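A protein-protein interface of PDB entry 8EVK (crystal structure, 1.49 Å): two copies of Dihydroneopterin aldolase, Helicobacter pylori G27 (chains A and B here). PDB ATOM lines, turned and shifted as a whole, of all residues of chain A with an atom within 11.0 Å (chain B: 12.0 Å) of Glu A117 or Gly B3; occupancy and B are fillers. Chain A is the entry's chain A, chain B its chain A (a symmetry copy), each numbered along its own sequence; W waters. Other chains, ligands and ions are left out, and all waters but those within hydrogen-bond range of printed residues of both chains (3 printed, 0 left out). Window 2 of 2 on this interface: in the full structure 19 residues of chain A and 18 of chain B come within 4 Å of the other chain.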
ATOM      1  N   LYS A   5       5.051 -29.528   7.871  1.00  0.00           N
ATOM      2  CA  LYS A   5       5.414 -28.229   8.422  1.00  0.00           C
ATOM      3  C   LYS A   5       5.401 -27.221   7.281  1.00  0.00           C
ATOM      4  O   LYS A   5       6.181 -27.354   6.333  1.00  0.00           O
ATOM      5  CB  LYS A   5       6.792 -28.295   9.082  1.00  0.00           C
ATOM      6  CG  LYS A   5       6.855 -29.219  10.300  1.00  0.00           C
ATOM      7  CD  LYS A   5       8.182 -29.077  11.042  1.00  0.00           C
ATOM      8  CE  LYS A   5       8.151 -29.776  12.396  1.00  0.00           C
ATOM      9  NZ  LYS A   5       9.417 -29.576  13.162  1.00  0.00           N
ATOM     10  N   PHE A  41       8.055 -14.473   7.716  1.00  0.00           N
ATOM     11  CA  PHE A  41       7.571 -15.846   7.659  1.00  0.00           C
ATOM     12  C   PHE A  41       6.585 -16.093   8.791  1.00  0.00           C
ATOM     13  O   PHE A  41       6.700 -15.504   9.870  1.00  0.00           O
ATOM     14  CB  PHE A  41       8.714 -16.844   7.764  1.00  0.00           C
ATOM     15  CG  PHE A  41       9.694 -16.770   6.627  1.00  0.00           C
ATOM     16  CD1 PHE A  41       9.395 -17.330   5.392  1.00  0.00           C
ATOM     17  CD2 PHE A  41      10.911 -16.143   6.800  1.00  0.00           C
ATOM     18  CE1 PHE A  41      10.314 -17.272   4.341  1.00  0.00           C
ATOM     19  CE2 PHE A  41      11.835 -16.081   5.760  1.00  0.00           C
ATOM     20  CZ  PHE A  41      11.534 -16.639   4.531  1.00  0.00           C
ATOM     21  N   THR A  43       3.369 -19.235  10.273  1.00  0.00           N
ATOM     22  CA  THR A  43       2.722 -20.529  10.126  1.00  0.00           C
ATOM     23  C   THR A  43       1.216 -20.419   9.920  1.00  0.00           C
ATOM     24  O   THR A  43       0.664 -21.161   9.106  1.00  0.00           O
ATOM     25  CB  THR A  43       3.052 -21.437  11.314  1.00  0.00           C
ATOM     26  OG1 THR A  43       2.992 -20.680  12.524  1.00  0.00           O
ATOM     27  CG2 THR A  43       4.461 -21.972  11.163  1.00  0.00           C
ATOM     28  N   LYS A  84       7.681  -6.740  13.948  1.00  0.00           N
ATOM     29  CA  LYS A  84       7.200  -7.829  14.800  1.00  0.00           C
ATOM     30  C   LYS A  84       6.020  -7.387  15.657  1.00  0.00           C
ATOM     31  O   LYS A  84       5.059  -8.145  15.839  1.00  0.00           O
ATOM     32  CB  LYS A  84       8.337  -8.374  15.667  1.00  0.00           C
ATOM     33  CG  LYS A  84       7.910  -9.366  16.757  1.00  0.00           C
ATOM     34  CD  LYS A  84       7.172 -10.583  16.206  1.00  0.00           C
ATOM     35  CE  LYS A  84       7.093 -11.663  17.279  1.00  0.00           C
ATOM     36  NZ  LYS A  84       6.486 -12.943  16.812  1.00  0.00           N
ATOM     37  N   LYS A  88       2.500  -9.786  15.065  1.00  0.00           N
ATOM     38  CA  LYS A  88       2.979 -10.664  16.127  1.00  0.00           C
ATOM     39  C   LYS A  88       3.024 -12.123  15.695  1.00  0.00           C
ATOM     40  O   LYS A  88       3.780 -12.908  16.274  1.00  0.00           O
ATOM     41  CB  LYS A  88       2.082 -10.531  17.359  1.00  0.00           C
ATOM     42  CG  LYS A  88       1.914  -9.108  17.867  1.00  0.00           C
ATOM     43  CD  LYS A  88       3.084  -8.647  18.707  1.00  0.00           C
ATOM     44  CE  LYS A  88       2.599  -7.715  19.824  1.00  0.00           C
ATOM     45  NZ  LYS A  88       1.744  -6.619  19.286  1.00  0.00           N
ATOM     46  N   GLU A  89       2.246 -12.492  14.679  1.00  0.00           N
ATOM     47  CA  GLU A  89       2.168 -13.872  14.222  1.00  0.00           C
ATOM     48  C   GLU A  89       3.442 -14.342  13.545  1.00  0.00           C
ATOM     49  O   GLU A  89       3.581 -15.542  13.294  1.00  0.00           O
ATOM     50  CB  GLU A  89       0.999 -14.026  13.241  1.00  0.00           C
ATOM     51  CG  GLU A  89       0.963 -12.967  12.140  1.00  0.00           C
ATOM     52  CD  GLU A  89       0.271 -11.680  12.574  1.00  0.00           C
ATOM     53  OE1 GLU A  89       0.504 -11.245  13.720  1.00  0.00           O
ATOM     54  OE2 GLU A  89      -0.490 -11.093  11.774  1.00  0.00           O
ATOM     55  N   ILE A  90       4.367 -13.445  13.211  1.00  0.00           N
ATOM     56  CA  ILE A  90       5.512 -13.897  12.439  1.00  0.00           C
ATOM     57  C   ILE A  90       6.415 -14.777  13.290  1.00  0.00           C
ATOM     58  O   ILE A  90       6.612 -14.546  14.493  1.00  0.00           O
ATOM     59  CB  ILE A  90       6.253 -12.735  11.758  1.00  0.00           C
ATOM     60  CG1 ILE A  90       6.898 -11.821  12.789  1.00  0.00           C
ATOM     61  CG2 ILE A  90       5.309 -11.967  10.840  1.00  0.00           C
ATOM     62  CD1 ILE A  90       7.847 -10.805  12.139  1.00  0.00           C
ATOM     63  N   THR A  91       6.925 -15.829  12.668  1.00  0.00           N
ATOM     64  CA  THR A  91       7.836 -16.766  13.284  1.00  0.00           C
ATOM     65  C   THR A  91       9.280 -16.482  12.922  1.00  0.00           C
ATOM     66  O   THR A  91      10.186 -16.943  13.618  1.00  0.00           O
ATOM     67  CB  THR A  91       7.468 -18.196  12.864  1.00  0.00           C
ATOM     68  OG1 THR A  91       7.438 -18.269  11.432  1.00  0.00           O
ATOM     69  CG2 THR A  91       6.081 -18.566  13.375  1.00  0.00           C
ATOM     70  N   GLU A  92       9.526 -15.713  11.857  1.00  0.00           N
ATOM     71  CA  GLU A  92      10.896 -15.453  11.452  1.00  0.00           C
ATOM     72  C   GLU A  92      10.879 -14.196  10.599  1.00  0.00           C
ATOM     73  O   GLU A  92       9.926 -13.966   9.851  1.00  0.00           O
ATOM     74  CB  GLU A  92      11.464 -16.644  10.672  1.00  0.00           C
ATOM     75  CG  GLU A  92      12.869 -16.439  10.101  1.00  0.00           C
ATOM     76  CD  GLU A  92      13.369 -17.650   9.331  1.00  0.00           C
ATOM     77  OE1 GLU A  92      12.825 -18.759   9.544  1.00  0.00           O
ATOM     78  OE2 GLU A  92      14.302 -17.494   8.509  1.00  0.00           O
ATOM     79  N   LEU A  93      11.889 -13.360  10.781  1.00  0.00           N
ATOM     80  CA  LEU A  93      12.036 -12.118  10.032  1.00  0.00           C
ATOM     81  C   LEU A  93      13.455 -12.071   9.510  1.00  0.00           C
ATOM     82  O   LEU A  93      14.402 -12.388  10.235  1.00  0.00           O
ATOM     83  CB  LEU A  93      11.778 -10.905  10.957  1.00  0.00           C
ATOM     84  CG  LEU A  93      12.001  -9.490  10.432  1.00  0.00           C
ATOM     85  CD1 LEU A  93      11.114  -8.545  11.186  1.00  0.00           C
ATOM     86  CD2 LEU A  93      13.460  -9.059  10.578  1.00  0.00           C
ATOM     87  N   LYS A 113      18.514 -11.467  11.118  1.00  0.00           N
ATOM     88  CA  LYS A 113      17.633 -12.620  11.028  1.00  0.00           C
ATOM     89  C   LYS A 113      17.171 -12.911  12.440  1.00  0.00           C
ATOM     90  O   LYS A 113      17.997 -13.131  13.329  1.00  0.00           O
ATOM     91  CB  LYS A 113      18.372 -13.841  10.491  1.00  0.00           C
ATOM     92  CG  LYS A 113      17.528 -15.086  10.378  1.00  0.00           C
ATOM     93  CD  LYS A 113      18.391 -16.284  10.007  1.00  0.00           C
ATOM     94  CE  LYS A 113      17.602 -17.582  10.041  1.00  0.00           C
ATOM     95  NZ  LYS A 113      18.314 -18.646   9.277  1.00  0.00           N
ATOM     96  N   ILE A 114      15.866 -12.923  12.641  1.00  0.00           N
ATOM     97  CA  ILE A 114      15.284 -13.134  13.956  1.00  0.00           C
ATOM     98  C   ILE A 114      14.355 -14.326  13.885  1.00  0.00           C
ATOM     99  O   ILE A 114      13.457 -14.366  13.040  1.00  0.00           O
ATOM    100  CB  ILE A 114      14.543 -11.895  14.450  1.00  0.00           C
ATOM    101  CG1 ILE A 114      15.470 -10.679  14.420  1.00  0.00           C
ATOM    102  CG2 ILE A 114      14.118 -12.115  15.891  1.00  0.00           C
ATOM    103  CD1 ILE A 114      14.850  -9.441  14.993  1.00  0.00           C
ATOM    104  N   CYS A 115      14.562 -15.292  14.784  1.00  0.00           N
ATOM    105  CA  CYS A 115      13.704 -16.460  14.894  1.00  0.00           C
ATOM    106  C   CYS A 115      12.961 -16.328  16.209  1.00  0.00           C
ATOM    107  O   CYS A 115      13.592 -16.207  17.264  1.00  0.00           O
ATOM    108  CB  CYS A 115      14.534 -17.737  14.890  1.00  0.00           C
ATOM    109  SG  CYS A 115      15.294 -18.051  13.271  1.00  0.00           S
ATOM    110  N   TYR A 116      11.641 -16.300  16.140  1.00  0.00           N
ATOM    111  CA  TYR A 116      10.795 -16.165  17.321  1.00  0.00           C
ATOM    112  C   TYR A 116      10.228 -17.528  17.711  1.00  0.00           C
ATOM    113  O   TYR A 116       9.688 -18.251  16.863  1.00  0.00           O
ATOM    114  CB  TYR A 116       9.653 -15.183  17.048  1.00  0.00           C
ATOM    115  CG  TYR A 116      10.085 -13.809  16.570  1.00  0.00           C
ATOM    116  CD1 TYR A 116      10.389 -12.804  17.476  1.00  0.00           C
ATOM    117  CD2 TYR A 116      10.186 -13.519  15.208  1.00  0.00           C
ATOM    118  CE1 TYR A 116      10.775 -11.550  17.058  1.00  0.00           C
ATOM    119  CE2 TYR A 116      10.586 -12.257  14.773  1.00  0.00           C
ATOM    120  CZ  TYR A 116      10.869 -11.278  15.706  1.00  0.00           C
ATOM    121  OH  TYR A 116      11.264 -10.025  15.299  1.00  0.00           O
ATOM    122  N   GLU A 117      10.340 -17.874  18.988  1.00  0.00           N
ATOM    123  CA  GLU A 117       9.742 -19.117  19.475  1.00  0.00           C
ATOM    124  C   GLU A 117       8.774 -18.843  20.622  1.00  0.00           C
ATOM    125  O   GLU A 117       8.756 -17.745  21.184  1.00  0.00           O
ATOM    126  CB  GLU A 117      10.819 -20.112  19.915  1.00  0.00           C
ATOM    127  CG  GLU A 117      10.358 -21.565  19.899  1.00  0.00           C
ATOM    128  CD  GLU A 117      11.433 -22.533  20.368  1.00  0.00           C
ATOM    129  OE1 GLU A 117      12.525 -22.065  20.761  1.00  0.00           O
ATOM    130  OE2 GLU A 117      11.183 -23.760  20.344  1.00  0.00           O
ATOM    131  N   GLY B   3      12.808 -16.775  23.881  1.00  0.00           N
ATOM    132  CA  GLY B   3      12.261 -17.391  22.684  1.00  0.00           C
ATOM    133  C   GLY B   3      12.598 -16.618  21.421  1.00  0.00           C
ATOM    134  O   GLY B   3      11.844 -16.636  20.445  1.00  0.00           O
ATOM    135  N   MET B   4      13.745 -15.943  21.439  1.00  0.00           N
ATOM    136  CA  MET B   4      14.139 -15.050  20.356  1.00  0.00           C
ATOM    137  C   MET B   4      15.628 -15.213  20.112  1.00  0.00           C
ATOM    138  O   MET B   4      16.432 -14.949  21.008  1.00  0.00           O
ATOM    139  CB  MET B   4      13.827 -13.602  20.740  1.00  0.00           C
ATOM    140  CG  MET B   4      14.026 -12.573  19.646  1.00  0.00           C
ATOM    141  SD  MET B   4      13.676 -10.925  20.301  1.00  0.00           S
ATOM    142  CE  MET B   4      13.510  -9.974  18.809  1.00  0.00           C
ATOM    143  N   LYS B   5      15.997 -15.627  18.901  1.00  0.00           N
ATOM    144  CA  LYS B   5      17.395 -15.766  18.515  1.00  0.00           C
ATOM    145  C   LYS B   5      17.662 -14.790  17.378  1.00  0.00           C
ATOM    146  O   LYS B   5      17.059 -14.912  16.308  1.00  0.00           O
ATOM    147  CB  LYS B   5      17.691 -17.204  18.086  1.00  0.00           C
ATOM    148  CG  LYS B   5      17.536 -18.232  19.209  1.00  0.00           C
ATOM    149  CD  LYS B   5      18.051 -19.606  18.785  1.00  0.00           C
ATOM    150  CE  LYS B   5      18.159 -20.560  19.968  1.00  0.00           C
ATOM    151  NZ  LYS B   5      18.736 -21.881  19.576  1.00  0.00           N
ATOM    152  N   THR B   6      18.547 -13.821  17.619  1.00  0.00           N
ATOM    153  CA  THR B   6      18.824 -12.719  16.700  1.00  0.00           C
ATOM    154  C   THR B   6      20.235 -12.877  16.160  1.00  0.00           C
ATOM    155  O   THR B   6      21.197 -12.934  16.936  1.00  0.00           O
ATOM    156  CB  THR B   6      18.716 -11.381  17.429  1.00  0.00           C
ATOM    157  OG1 THR B   6      17.379 -11.187  17.909  1.00  0.00           O
ATOM    158  CG2 THR B   6      19.080 -10.241  16.503  1.00  0.00           C
ATOM    159  N   LYS B   7      20.365 -12.917  14.837  1.00  0.00           N
ATOM    160  CA  LYS B   7      21.655 -13.080  14.187  1.00  0.00           C
ATOM    161  C   LYS B   7      21.878 -11.840  13.342  1.00  0.00           C
ATOM    162  O   LYS B   7      21.176 -11.638  12.342  1.00  0.00           O
ATOM    163  CB  LYS B   7      21.637 -14.325  13.308  1.00  0.00           C
ATOM    164  CG  LYS B   7      22.959 -14.682  12.660  1.00  0.00           C
ATOM    165  CD  LYS B   7      22.723 -15.793  11.649  1.00  0.00           C
ATOM    166  CE  LYS B   7      23.997 -16.523  11.300  1.00  0.00           C
ATOM    167  NZ  LYS B   7      23.685 -17.652  10.368  1.00  0.00           N
HETATM  168  O   HOH W   1       8.891 -15.177  20.699  1.00  0.00           O
HETATM  169  O   HOH W   2      18.306 -16.280  13.942  1.00  0.00           O
HETATM  170  O   HOH W   3      14.011 -18.455  18.775  1.00  0.00           O
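O of Lys A113 is in hydrogen-bond range of N of Lys B7. The backbone NH of Cys A115 lies within hydrogen-bond range of the backbone carbonyl oxygen of Lys B5. The backbone carbonyl oxygen of Gly B3 is in hydrogen-bond range of the backbone NH of Glu A117, 2.4 Å away.
The backbone carbonyl oxygen (O) of Leu A93 lies within hydrogen-bond range of the backbone NH (N) of Ile A114, at 2.9 Å. The backbone carbonyl oxygen (O) of Thr A91 sits at hydrogen-bond distance from the backbone NH (N) of Tyr A116 (3.0 Å).
Among the printed residues, pairs that only touch across the chains: Lys A113 with Lys B5 (3.6 Å), Lys A113 with Thr B6 (3.5 Å), Ile A114 with Met B4 (3.7 Å), Ile A114 with Lys B5 (3.4 Å), Ile A114 with Thr B6 (3.9 Å), Cys A115 with Gly B3 (3.7 Å), Cys A115 with Met B4 (3.3 Å), Tyr A116 with Gly B3 (3.3 Å) and Tyr A116 with Met B4 (3.6 Å).
Of chain B, only Gly B3 (2.4 Å) comes within 4 Å of Glu A117. Gly B3 touches just these residues of chain A: Cys A115, Tyr A116 and Glu A117. Printed residues of chain A within 4 Å of Lys B5: Lys A113 (3.6 Å), Ile A114 (3.4 Å) and Cys A115 (2.9 Å). Of the printed residues of chain A, Met B4 touches Ile A114 (3.7 Å), Cys A115 (3.3 Å) and Tyr A116 (3.6 Å). Of the printed residues of chain B, Ile A114 touches Met B4 (3.7 Å), Lys B5 (3.4 Å) and Thr B6 (3.9 Å). Printed residues of chain B within 4 Å of Tyr A116: Gly B3 (3.3 Å) and Met B4 (3.6 Å). Leu A93 touches none of the printed residues of chain B. The nearest residue of chain B that does not touch Glu A117 is Met B4 (4.6 Å). The nearest residue of chain A that does not touch Gly B3 is Ile A114 (6.8 Å).
Printed residues of chain A that touch a printed residue of chain B: Lys A113, Ile A114, Cys A115, Tyr A116 and Glu A117. Hydrophobic or aromatic side chains of chain B that line the printed part of chain A: Met B4.
Position printed for both chains: 5. Of the 12 pairs that touch across the chains among the printed residues, none has its exchanged pair printed and touching as well.
Water W1 lies within hydrogen-bond range of the backbone carbonyl oxygen (O) of Glu A117 (2.6 Å) and the backbone carbonyl oxygen (O) of Gly B3 (3.3 Å). Water W3 lies within hydrogen-bond range of the backbone carbonyl oxygen (O) of Cys A115 (2.7 Å), the backbone carbonyl oxygen (O) of Gly B3 (3.3 Å) and the backbone NH (N) of Lys B5 (3.5 Å). Water W2 lies within hydrogen-bond range of the backbone carbonyl oxygen (O) of Lys B5, the backbone carbonyl oxygen (O) of Lys A113 and the side-chain sulfur (SG) of Cys A115.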
